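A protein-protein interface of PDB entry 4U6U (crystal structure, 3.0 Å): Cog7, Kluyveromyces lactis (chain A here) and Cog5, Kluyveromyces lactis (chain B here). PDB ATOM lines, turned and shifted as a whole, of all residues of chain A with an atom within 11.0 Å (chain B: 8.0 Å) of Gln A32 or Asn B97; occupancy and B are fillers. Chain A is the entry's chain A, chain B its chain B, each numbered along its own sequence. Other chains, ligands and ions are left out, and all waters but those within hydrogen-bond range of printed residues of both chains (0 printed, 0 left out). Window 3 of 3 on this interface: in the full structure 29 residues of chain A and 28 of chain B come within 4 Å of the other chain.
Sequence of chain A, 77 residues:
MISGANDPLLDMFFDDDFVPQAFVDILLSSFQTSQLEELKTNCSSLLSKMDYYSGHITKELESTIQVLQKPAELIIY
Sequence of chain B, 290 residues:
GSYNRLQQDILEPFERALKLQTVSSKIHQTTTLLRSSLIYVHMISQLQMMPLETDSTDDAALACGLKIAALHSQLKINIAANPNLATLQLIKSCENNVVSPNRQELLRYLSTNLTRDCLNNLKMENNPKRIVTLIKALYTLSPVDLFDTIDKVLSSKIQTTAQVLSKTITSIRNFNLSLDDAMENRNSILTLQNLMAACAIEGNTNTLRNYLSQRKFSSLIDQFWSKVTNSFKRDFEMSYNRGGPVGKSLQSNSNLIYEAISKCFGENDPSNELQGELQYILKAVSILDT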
ATOM      1  N   ASP A  25     -14.908 -15.880  -3.229  1.00  0.00           N
ATOM      2  CA  ASP A  25     -13.946 -14.896  -3.677  1.00  0.00           C
ATOM      3  C   ASP A  25     -14.615 -13.850  -4.570  1.00  0.00           C
ATOM      4  O   ASP A  25     -14.403 -12.649  -4.387  1.00  0.00           O
ATOM      5  CB  ASP A  25     -12.796 -15.586  -4.418  1.00  0.00           C
ATOM      6  CG  ASP A  25     -11.541 -14.733  -4.480  1.00  0.00           C
ATOM      7  OD1 ASP A  25     -11.370 -13.862  -3.596  1.00  0.00           O
ATOM      8  OD2 ASP A  25     -10.729 -14.940  -5.407  1.00  0.00           O
ATOM      9  N   ILE A  26     -15.427 -14.299  -5.524  1.00  0.00           N
ATOM     10  CA  ILE A  26     -16.063 -13.378  -6.467  1.00  0.00           C
ATOM     11  C   ILE A  26     -17.110 -12.572  -5.696  1.00  0.00           C
ATOM     12  O   ILE A  26     -17.339 -11.400  -5.972  1.00  0.00           O
ATOM     13  CB  ILE A  26     -16.704 -14.109  -7.710  1.00  0.00           C
ATOM     14  CG1 ILE A  26     -17.989 -14.864  -7.317  1.00  0.00           C
ATOM     15  CG2 ILE A  26     -15.687 -15.031  -8.369  1.00  0.00           C
ATOM     16  CD1 ILE A  26     -18.677 -15.674  -8.437  1.00  0.00           C
ATOM     17  N   LEU A  27     -17.730 -13.208  -4.712  1.00  0.00           N
ATOM     18  CA  LEU A  27     -18.834 -12.600  -3.987  1.00  0.00           C
ATOM     19  C   LEU A  27     -18.410 -11.386  -3.172  1.00  0.00           C
ATOM     20  O   LEU A  27     -18.880 -10.268  -3.408  1.00  0.00           O
ATOM     21  CB  LEU A  27     -19.490 -13.643  -3.073  1.00  0.00           C
ATOM     22  CG  LEU A  27     -20.502 -13.079  -2.075  1.00  0.00           C
ATOM     23  CD1 LEU A  27     -21.668 -12.475  -2.816  1.00  0.00           C
ATOM     24  CD2 LEU A  27     -20.978 -14.135  -1.076  1.00  0.00           C
ATOM     25  N   LEU A  28     -17.482 -11.613  -2.250  1.00  0.00           N
ATOM     26  CA  LEU A  28     -17.012 -10.582  -1.338  1.00  0.00           C
ATOM     27  C   LEU A  28     -16.489  -9.342  -2.067  1.00  0.00           C
ATOM     28  O   LEU A  28     -16.563  -8.226  -1.541  1.00  0.00           O
ATOM     29  CB  LEU A  28     -15.914 -11.160  -0.460  1.00  0.00           C
ATOM     30  CG  LEU A  28     -16.237 -11.744   0.908  1.00  0.00           C
ATOM     31  CD1 LEU A  28     -17.687 -12.095   1.003  1.00  0.00           C
ATOM     32  CD2 LEU A  28     -15.366 -12.953   1.170  1.00  0.00           C
ATOM     33  N   SER A  29     -15.951  -9.546  -3.267  1.00  0.00           N
ATOM     34  CA  SER A  29     -15.523  -8.453  -4.126  1.00  0.00           C
ATOM     35  C   SER A  29     -16.709  -7.645  -4.638  1.00  0.00           C
ATOM     36  O   SER A  29     -17.212  -7.910  -5.726  1.00  0.00           O
ATOM     37  CB  SER A  29     -14.725  -9.010  -5.285  1.00  0.00           C
ATOM     38  OG  SER A  29     -13.587  -9.666  -4.776  1.00  0.00           O
ATOM     39  N   SER A  30     -17.144  -6.656  -3.859  1.00  0.00           N
ATOM     40  CA  SER A  30     -18.225  -5.763  -4.286  1.00  0.00           C
ATOM     41  C   SER A  30     -18.488  -4.434  -3.522  1.00  0.00           C
ATOM     42  O   SER A  30     -19.656  -4.029  -3.462  1.00  0.00           O
ATOM     43  CB  SER A  30     -19.541  -6.568  -4.288  1.00  0.00           C
ATOM     44  OG  SER A  30     -20.672  -5.744  -4.521  1.00  0.00           O
ATOM     45  N   PHE A  31     -17.506  -3.737  -2.929  1.00  0.00           N
ATOM     46  CA  PHE A  31     -16.146  -4.160  -2.579  1.00  0.00           C
ATOM     47  C   PHE A  31     -16.011  -3.735  -1.121  1.00  0.00           C
ATOM     48  O   PHE A  31     -17.023  -3.592  -0.437  1.00  0.00           O
ATOM     49  CB  PHE A  31     -15.047  -3.512  -3.447  1.00  0.00           C
ATOM     50  CG  PHE A  31     -15.045  -1.991  -3.435  1.00  0.00           C
ATOM     51  CD1 PHE A  31     -15.945  -1.260  -4.201  1.00  0.00           C
ATOM     52  CD2 PHE A  31     -14.113  -1.296  -2.670  1.00  0.00           C
ATOM     53  CE1 PHE A  31     -15.930   0.127  -4.184  1.00  0.00           C
ATOM     54  CE2 PHE A  31     -14.095   0.086  -2.651  1.00  0.00           C
ATOM     55  CZ  PHE A  31     -15.003   0.797  -3.408  1.00  0.00           C
ATOM     56  N   GLN A  32     -14.788  -3.535  -0.632  1.00  0.00           N
ATOM     57  CA  GLN A  32     -14.579  -3.354   0.809  1.00  0.00           C
ATOM     58  C   GLN A  32     -14.734  -1.893   1.223  1.00  0.00           C
ATOM     59  O   GLN A  32     -15.485  -1.164   0.579  1.00  0.00           O
ATOM     60  CB  GLN A  32     -13.187  -3.847   1.208  1.00  0.00           C
ATOM     61  CG  GLN A  32     -12.038  -3.120   0.515  1.00  0.00           C
ATOM     62  CD  GLN A  32     -11.060  -2.512   1.495  1.00  0.00           C
ATOM     63  OE1 GLN A  32     -11.278  -2.536   2.707  1.00  0.00           O
ATOM     64  NE2 GLN A  32      -9.978  -1.954   0.974  1.00  0.00           N
ATOM     65  N   THR A  33     -13.976  -1.460   2.234  1.00  0.00           N
ATOM     66  CA  THR A  33     -14.027  -0.090   2.759  1.00  0.00           C
ATOM     67  C   THR A  33     -15.429   0.455   3.066  1.00  0.00           C
ATOM     68  O   THR A  33     -16.288   0.538   2.193  1.00  0.00           O
ATOM     69  CB  THR A  33     -13.327   0.931   1.799  1.00  0.00           C
ATOM     70  OG1 THR A  33     -13.835   0.782   0.463  1.00  0.00           O
ATOM     71  CG2 THR A  33     -11.810   0.739   1.782  1.00  0.00           C
ATOM     72  N   SER A  34     -15.633   0.867   4.316  1.00  0.00           N
ATOM     73  CA  SER A  34     -16.891   1.469   4.783  1.00  0.00           C
ATOM     74  C   SER A  34     -18.125   0.644   4.407  1.00  0.00           C
ATOM     75  O   SER A  34     -18.904   0.257   5.283  1.00  0.00           O
ATOM     76  CB  SER A  34     -17.036   2.907   4.256  1.00  0.00           C
ATOM     77  OG  SER A  34     -16.967   2.973   2.841  1.00  0.00           O
ATOM     78  N   GLN A  35     -18.299   0.374   3.112  1.00  0.00           N
ATOM     79  CA  GLN A  35     -19.463  -0.357   2.619  1.00  0.00           C
ATOM     80  C   GLN A  35     -19.255  -1.864   2.806  1.00  0.00           C
ATOM     81  O   GLN A  35     -19.806  -2.676   2.071  1.00  0.00           O
ATOM     82  CB  GLN A  35     -19.726  -0.012   1.137  1.00  0.00           C
ATOM     83  CG  GLN A  35     -18.736  -0.623   0.131  1.00  0.00           C
ATOM     84  CD  GLN A  35     -19.035  -0.254  -1.317  1.00  0.00           C
ATOM     85  OE1 GLN A  35     -19.355  -1.125  -2.133  1.00  0.00           O
ATOM     86  NE2 GLN A  35     -18.910   1.039  -1.647  1.00  0.00           N
ATOM     87  N   LEU A  36     -18.445  -2.212   3.806  1.00  0.00           N
ATOM     88  CA  LEU A  36     -18.263  -3.586   4.255  1.00  0.00           C
ATOM     89  C   LEU A  36     -19.270  -3.947   5.364  1.00  0.00           C
ATOM     90  O   LEU A  36     -19.235  -5.046   5.907  1.00  0.00           O
ATOM     91  CB  LEU A  36     -16.812  -3.825   4.710  1.00  0.00           C
ATOM     92  CG  LEU A  36     -16.129  -3.276   5.978  1.00  0.00           C
ATOM     93  CD1 LEU A  36     -16.390  -1.778   6.268  1.00  0.00           C
ATOM     94  CD2 LEU A  36     -16.429  -4.140   7.197  1.00  0.00           C
ATOM     95  N   GLU A  37     -20.131  -2.999   5.723  1.00  0.00           N
ATOM     96  CA  GLU A  37     -21.252  -3.251   6.630  1.00  0.00           C
ATOM     97  C   GLU A  37     -22.428  -3.677   5.765  1.00  0.00           C
ATOM     98  O   GLU A  37     -23.250  -4.515   6.144  1.00  0.00           O
ATOM     99  CB  GLU A  37     -21.608  -2.011   7.453  1.00  0.00           C
ATOM    100  CG  GLU A  37     -20.844  -1.877   8.753  1.00  0.00           C
ATOM    101  CD  GLU A  37     -21.500  -2.631   9.880  1.00  0.00           C
ATOM    102  OE1 GLU A  37     -22.678  -3.012   9.721  1.00  0.00           O
ATOM    103  OE2 GLU A  37     -20.844  -2.847  10.920  1.00  0.00           O
ATOM    104  N   GLU A  38     -22.457  -3.077   4.579  1.00  0.00           N
ATOM    105  CA  GLU A  38     -23.432  -3.348   3.537  1.00  0.00           C
ATOM    106  C   GLU A  38     -23.339  -4.816   3.153  1.00  0.00           C
ATOM    107  O   GLU A  38     -24.298  -5.574   3.305  1.00  0.00           O
ATOM    108  CB  GLU A  38     -23.153  -2.469   2.312  1.00  0.00           C
ATOM    109  CG  GLU A  38     -23.023  -0.975   2.599  1.00  0.00           C
ATOM    110  CD  GLU A  38     -24.336  -0.239   2.461  1.00  0.00           C
ATOM    111  OE1 GLU A  38     -24.316   1.001   2.314  1.00  0.00           O
ATOM    112  OE2 GLU A  38     -25.392  -0.903   2.494  1.00  0.00           O
ATOM    113  N   LEU A  39     -22.170  -5.203   2.648  1.00  0.00           N
ATOM    114  CA  LEU A  39     -21.918  -6.583   2.264  1.00  0.00           C
ATOM    115  C   LEU A  39     -21.900  -7.513   3.484  1.00  0.00           C
ATOM    116  O   LEU A  39     -21.966  -8.728   3.337  1.00  0.00           O
ATOM    117  CB  LEU A  39     -20.604  -6.695   1.473  1.00  0.00           C
ATOM    118  CG  LEU A  39     -20.673  -6.534  -0.061  1.00  0.00           C
ATOM    119  CD1 LEU A  39     -19.433  -5.817  -0.596  1.00  0.00           C
ATOM    120  CD2 LEU A  39     -20.866  -7.876  -0.793  1.00  0.00           C
ATOM    121  N   LYS A  40     -21.822  -6.964   4.691  1.00  0.00           N
ATOM    122  CA  LYS A  40     -21.813  -7.825   5.872  1.00  0.00           C
ATOM    123  C   LYS A  40     -23.220  -8.338   6.163  1.00  0.00           C
ATOM    124  O   LYS A  40     -23.392  -9.482   6.564  1.00  0.00           O
ATOM    125  CB  LYS A  40     -21.240  -7.101   7.101  1.00  0.00           C
ATOM    126  CG  LYS A  40     -21.287  -7.929   8.394  1.00  0.00           C
ATOM    127  CD  LYS A  40     -20.365  -7.397   9.513  1.00  0.00           C
ATOM    128  CE  LYS A  40     -20.473  -5.900   9.737  1.00  0.00           C
ATOM    129  NZ  LYS A  40     -19.491  -5.437  10.763  1.00  0.00           N
ATOM    130  N   VAL B  41     -14.315  -9.902   9.210  1.00  0.00           N
ATOM    131  CA  VAL B  41     -14.883  -8.568   9.034  1.00  0.00           C
ATOM    132  C   VAL B  41     -15.436  -7.933  10.326  1.00  0.00           C
ATOM    133  O   VAL B  41     -15.179  -6.756  10.615  1.00  0.00           O
ATOM    134  CB  VAL B  41     -15.973  -8.613   7.969  1.00  0.00           C
ATOM    135  CG1 VAL B  41     -17.031  -7.528   8.193  1.00  0.00           C
ATOM    136  CG2 VAL B  41     -15.324  -8.503   6.599  1.00  0.00           C
ATOM    137  N   ILE B  44     -12.515  -6.678  12.067  1.00  0.00           N
ATOM    138  CA  ILE B  44     -12.044  -5.448  11.472  1.00  0.00           C
ATOM    139  C   ILE B  44     -12.950  -4.274  11.831  1.00  0.00           C
ATOM    140  O   ILE B  44     -12.485  -3.172  12.112  1.00  0.00           O
ATOM    141  CB  ILE B  44     -11.928  -5.616   9.965  1.00  0.00           C
ATOM    142  CG1 ILE B  44     -10.695  -6.467   9.696  1.00  0.00           C
ATOM    143  CG2 ILE B  44     -11.814  -4.279   9.262  1.00  0.00           C
ATOM    144  CD1 ILE B  44     -10.097  -6.247   8.365  1.00  0.00           C
ATOM    145  N   GLN B  48     -11.473  -0.999  13.934  1.00  0.00           N
ATOM    146  CA  GLN B  48     -11.612   0.413  13.612  1.00  0.00           C
ATOM    147  C   GLN B  48     -12.450   1.171  14.632  1.00  0.00           C
ATOM    148  O   GLN B  48     -12.565   2.395  14.555  1.00  0.00           O
ATOM    149  CB  GLN B  48     -12.269   0.580  12.246  1.00  0.00           C
ATOM    150  CG  GLN B  48     -11.468   0.104  11.074  1.00  0.00           C
ATOM    151  CD  GLN B  48     -12.262   0.220   9.794  1.00  0.00           C
ATOM    152  OE1 GLN B  48     -13.368  -0.325   9.688  1.00  0.00           O
ATOM    153  NE2 GLN B  48     -11.721   0.956   8.824  1.00  0.00           N
ATOM    154  N   GLN B  89      -8.887 -12.049  -2.583  1.00  0.00           N
ATOM    155  CA  GLN B  89      -8.580 -10.655  -2.979  1.00  0.00           C
ATOM    156  C   GLN B  89      -9.437  -9.514  -2.430  1.00  0.00           C
ATOM    157  O   GLN B  89      -9.425  -8.415  -2.989  1.00  0.00           O
ATOM    158  CB  GLN B  89      -8.558 -10.518  -4.508  1.00  0.00           C
ATOM    159  CG  GLN B  89      -7.243 -10.959  -5.135  1.00  0.00           C
ATOM    160  CD  GLN B  89      -7.188 -10.674  -6.623  1.00  0.00           C
ATOM    161  OE1 GLN B  89      -8.221 -10.510  -7.273  1.00  0.00           O
ATOM    162  NE2 GLN B  89      -5.978 -10.588  -7.166  1.00  0.00           N
ATOM    163  N   LEU B  90     -10.156  -9.760  -1.345  1.00  0.00           N
ATOM    164  CA  LEU B  90     -10.955  -8.726  -0.702  1.00  0.00           C
ATOM    165  C   LEU B  90     -10.687  -8.818   0.786  1.00  0.00           C
ATOM    166  O   LEU B  90     -11.077  -7.956   1.559  1.00  0.00           O
ATOM    167  CB  LEU B  90     -12.437  -8.867  -1.035  1.00  0.00           C
ATOM    168  CG  LEU B  90     -13.048  -7.681  -1.802  1.00  0.00           C
ATOM    169  CD1 LEU B  90     -13.245  -6.504  -0.890  1.00  0.00           C
ATOM    170  CD2 LEU B  90     -12.227  -7.255  -3.030  1.00  0.00           C
ATOM    171  N   ILE B  91     -10.057  -9.914   1.181  1.00  0.00           N
ATOM    172  CA  ILE B  91      -9.535 -10.036   2.525  1.00  0.00           C
ATOM    173  C   ILE B  91      -8.121  -9.484   2.574  1.00  0.00           C
ATOM    174  O   ILE B  91      -7.721  -8.863   3.554  1.00  0.00           O
ATOM    175  CB  ILE B  91      -9.536 -11.501   2.987  1.00  0.00           C
ATOM    176  CG1 ILE B  91     -10.336 -11.652   4.261  1.00  0.00           C
ATOM    177  CG2 ILE B  91      -8.127 -12.030   3.229  1.00  0.00           C
ATOM    178  CD1 ILE B  91     -10.599 -13.097   4.579  1.00  0.00           C
ATOM    179  N   LYS B  92      -7.367  -9.693   1.502  1.00  0.00           N
ATOM    180  CA  LYS B  92      -6.061  -9.074   1.375  1.00  0.00           C
ATOM    181  C   LYS B  92      -6.224  -7.564   1.266  1.00  0.00           C
ATOM    182  O   LYS B  92      -5.501  -6.816   1.918  1.00  0.00           O
ATOM    183  CB  LYS B  92      -5.294  -9.651   0.182  1.00  0.00           C
ATOM    184  CG  LYS B  92      -4.635 -11.014   0.457  1.00  0.00           C
ATOM    185  CD  LYS B  92      -4.192 -11.709  -0.839  1.00  0.00           C
ATOM    186  CE  LYS B  92      -3.344 -12.963  -0.576  1.00  0.00           C
ATOM    187  NZ  LYS B  92      -2.031 -12.665   0.093  1.00  0.00           N
ATOM    188  N   SER B  93      -7.201  -7.116   0.482  1.00  0.00           N
ATOM    189  CA  SER B  93      -7.394  -5.687   0.257  1.00  0.00           C
ATOM    190  C   SER B  93      -7.731  -4.900   1.517  1.00  0.00           C
ATOM    191  O   SER B  93      -7.581  -3.682   1.541  1.00  0.00           O
ATOM    192  CB  SER B  93      -8.493  -5.461  -0.778  1.00  0.00           C
ATOM    193  OG  SER B  93      -8.047  -5.854  -2.061  1.00  0.00           O
ATOM    194  N   CYS B  94      -8.199  -5.569   2.559  1.00  0.00           N
ATOM    195  CA  CYS B  94      -8.373  -4.873   3.825  1.00  0.00           C
ATOM    196  C   CYS B  94      -7.186  -5.232   4.737  1.00  0.00           C
ATOM    197  O   CYS B  94      -6.907  -4.522   5.703  1.00  0.00           O
ATOM    198  CB  CYS B  94      -9.749  -5.135   4.461  1.00  0.00           C
ATOM    199  SG  CYS B  94     -10.189  -6.778   4.987  1.00  0.00           S
ATOM    200  N   GLU B  95      -6.516  -6.350   4.448  1.00  0.00           N
ATOM    201  CA  GLU B  95      -5.356  -6.777   5.236  1.00  0.00           C
ATOM    202  C   GLU B  95      -4.238  -5.733   5.209  1.00  0.00           C
ATOM    203  O   GLU B  95      -3.485  -5.593   6.180  1.00  0.00           O
ATOM    204  CB  GLU B  95      -4.817  -8.122   4.728  1.00  0.00           C
ATOM    205  CG  GLU B  95      -3.504  -8.597   5.380  1.00  0.00           C
ATOM    206  CD  GLU B  95      -3.633  -9.037   6.830  1.00  0.00           C
ATOM    207  OE1 GLU B  95      -2.696  -8.751   7.611  1.00  0.00           O
ATOM    208  OE2 GLU B  95      -4.654  -9.664   7.188  1.00  0.00           O
ATOM    209  N   ASN B  96      -4.124  -5.004   4.101  1.00  0.00           N
ATOM    210  CA  ASN B  96      -3.105  -3.959   4.002  1.00  0.00           C
ATOM    211  C   ASN B  96      -3.700  -2.546   4.032  1.00  0.00           C
ATOM    212  O   ASN B  96      -2.968  -1.570   4.160  1.00  0.00           O
ATOM    213  CB  ASN B  96      -2.222  -4.157   2.760  1.00  0.00           C
ATOM    214  CG  ASN B  96      -2.924  -3.818   1.471  1.00  0.00           C
ATOM    215  OD1 ASN B  96      -3.028  -2.652   1.094  1.00  0.00           O
ATOM    216  ND2 ASN B  96      -3.385  -4.840   0.767  1.00  0.00           N
ATOM    217  N   ASN B  97      -5.022  -2.436   3.928  1.00  0.00           N
ATOM    218  CA  ASN B  97      -5.674  -1.127   3.925  1.00  0.00           C
ATOM    219  C   ASN B  97      -6.188  -0.720   5.290  1.00  0.00           C
ATOM    220  O   ASN B  97      -6.390   0.461   5.554  1.00  0.00           O
ATOM    221  CB  ASN B  97      -6.856  -1.102   2.959  1.00  0.00           C
ATOM    222  CG  ASN B  97      -6.441  -0.827   1.544  1.00  0.00           C
ATOM    223  OD1 ASN B  97      -5.288  -0.481   1.284  1.00  0.00           O
ATOM    224  ND2 ASN B  97      -7.385  -0.937   0.618  1.00  0.00           N
ATOM    225  N   VAL B  98      -6.415  -1.696   6.155  1.00  0.00           N
ATOM    226  CA  VAL B  98      -6.924  -1.400   7.480  1.00  0.00           C
ATOM    227  C   VAL B  98      -6.003  -1.988   8.547  1.00  0.00           C
ATOM    228  O   VAL B  98      -5.588  -1.268   9.458  1.00  0.00           O
ATOM    229  CB  VAL B  98      -8.371  -1.916   7.663  1.00  0.00           C
ATOM    230  CG1 VAL B  98      -8.881  -1.584   9.048  1.00  0.00           C
ATOM    231  CG2 VAL B  98      -9.288  -1.306   6.614  1.00  0.00           C
ATOM    232  N   VAL B  99      -5.643  -3.266   8.428  1.00  0.00           N
ATOM    233  CA  VAL B  99      -4.936  -3.916   9.533  1.00  0.00           C
ATOM    234  C   VAL B  99      -3.438  -3.671   9.469  1.00  0.00           C
ATOM    235  O   VAL B  99      -2.839  -3.393  10.493  1.00  0.00           O
ATOM    236  CB  VAL B  99      -5.223  -5.447   9.624  1.00  0.00           C
ATOM    237  CG1 VAL B  99      -6.083  -5.900   8.480  1.00  0.00           C
ATOM    238  CG2 VAL B  99      -3.927  -6.275   9.753  1.00  0.00           C
ATOM    239  N   SER B 100      -2.827  -3.763   8.296  1.00  0.00           N
ATOM    240  CA  SER B 100      -1.397  -3.471   8.201  1.00  0.00           C
ATOM    241  C   SER B 100      -1.033  -2.006   8.587  1.00  0.00           C
ATOM    242  O   SER B 100       0.053  -1.758   9.112  1.00  0.00           O
ATOM    243  CB  SER B 100      -0.896  -3.792   6.792  1.00  0.00           C
ATOM    244  OG  SER B 100       0.335  -3.141   6.526  1.00  0.00           O
ATOM    245  N   PRO B 101      -1.932  -1.033   8.331  1.00  0.00           N
ATOM    246  CA  PRO B 101      -1.700   0.289   8.919  1.00  0.00           C
ATOM    247  C   PRO B 101      -1.971   0.372  10.421  1.00  0.00           C
ATOM    248  O   PRO B 101      -1.107   0.845  11.157  1.00  0.00           O
ATOM    249  CB  PRO B 101      -2.686   1.179   8.163  1.00  0.00           C
ATOM    250  CG  PRO B 101      -2.888   0.505   6.883  1.00  0.00           C
ATOM    251  CD  PRO B 101      -2.887  -0.951   7.213  1.00  0.00           C
ATOM    252  N   ASN B 102      -3.148  -0.061  10.865  1.00  0.00           N
ATOM    253  CA  ASN B 102      -3.471  -0.104  12.295  1.00  0.00           C
ATOM    254  C   ASN B 102      -2.373  -0.800  13.095  1.00  0.00           C
ATOM    255  O   ASN B 102      -2.057  -0.411  14.219  1.00  0.00           O
ATOM    256  CB  ASN B 102      -4.810  -0.807  12.523  1.00  0.00           C
ATOM    257  CG  ASN B 102      -5.257  -0.772  13.986  1.00  0.00           C
ATOM    258  OD1 ASN B 102      -4.713  -1.488  14.839  1.00  0.00           O
ATOM    259  ND2 ASN B 102      -6.265   0.058  14.279  1.00  0.00           N
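Ile A26 touches none of the printed residues of chain B.
Of the printed residues of chain B, Leu A28 touches Leu B90 (3.6 Å).
Printed residues of chain B within 4 Å of Ser A29: Leu B90 (3.3 Å).
Gln A32 touches just these residues of chain B: Leu B90, Ser B93, Cys B94 and Asn B97.
Leu A39 touches none of the printed residues of chain B.
Printed residues of chain A within 4 Å of Val B41: Leu A36 and Lys A40.
Of the printed residues of chain A, Gln B89 touches Asp A25 (3.2 Å).
Of the printed residues of chain A, Leu B90 touches Leu A28, Ser A29, Phe A31 and Gln A32.
No residue of chain A comes within 4 Å of Asn B96.
The nearest residue of chain B that does not touch Gln A32 is Val B98 (4.6 Å).
The nearest residue of chain A that does not touch Asn B97 is Thr A33 (4.9 Å).
The nearest printed residue of chain B that does not touch Ser A29 is Gln B89 (4.7 Å).
The backbone carbonyl oxygen (O) of Ser B93 is in hydrogen-bond range of the side-chain amide nitrogen (NE2) of Gln A32.
OD1 of Asp A25 is in hydrogen-bond range of N of Gln B89.
NE2 of Gln A32 lies close to ND2 of Asn B97.
The side-chain sulfur (SG) of Cys B94 lies within hydrogen-bond range of the backbone carbonyl oxygen (O) of Leu B90.
The side-chain carboxylate (OE2) of Glu A37 lies within salt-bridge range of the side-chain amino group (NZ) of Lys A40 (2.9 Å).
OD1 of Asn B96 sits close to OD1 of Asn B97, 3.1 Å away.
N of Phe A31 lies within hydrogen-bond range of OE1 of Gln A35 (3.3 Å).
The backbone carbonyl oxygen of Ser B93 sits at hydrogen-bond distance from the side-chain amide nitrogen of Asn B97 (2.9 Å).
The backbone carbonyl oxygen (O) of Ile B91 is in hydrogen-bond range of the side-chain sulfur (SG) of Cys B94, 3.5 Å away.
Leu A28 touches Leu B90.
Leu B90 touches Ser A29 (CD2 to OG, 3.3 Å).
Phe A31 touches Leu B90 (C to CD1, 3.9 Å).
N of Gln A32 touches CD1 of Leu B90, at 3.4 Å.
OE1 of Gln A32 touches CB of Cys B94 (3.5 Å).
Leu A36 touches Val B41 (CD2 to CG1, 3.6 Å).
CD of Lys A40 touches CG1 of Val B41 (3.6 Å).
Of the 17 printed residues of chain B, 6 touch a printed residue of chain A.
Printed residues of chain B that touch a printed residue of chain A: Val B41, Gln B89, Leu B90, Ser B93, Cys B94 and Asn B97.
Hydrophobic or aromatic side chains of chain B that line the printed part of chain A: Val B41 and Leu B90.
Hydrophobic or aromatic side chains of chain A that line the printed part of chain B: Leu A36.
Among the printed residues, 10 pairs touch across the chains.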
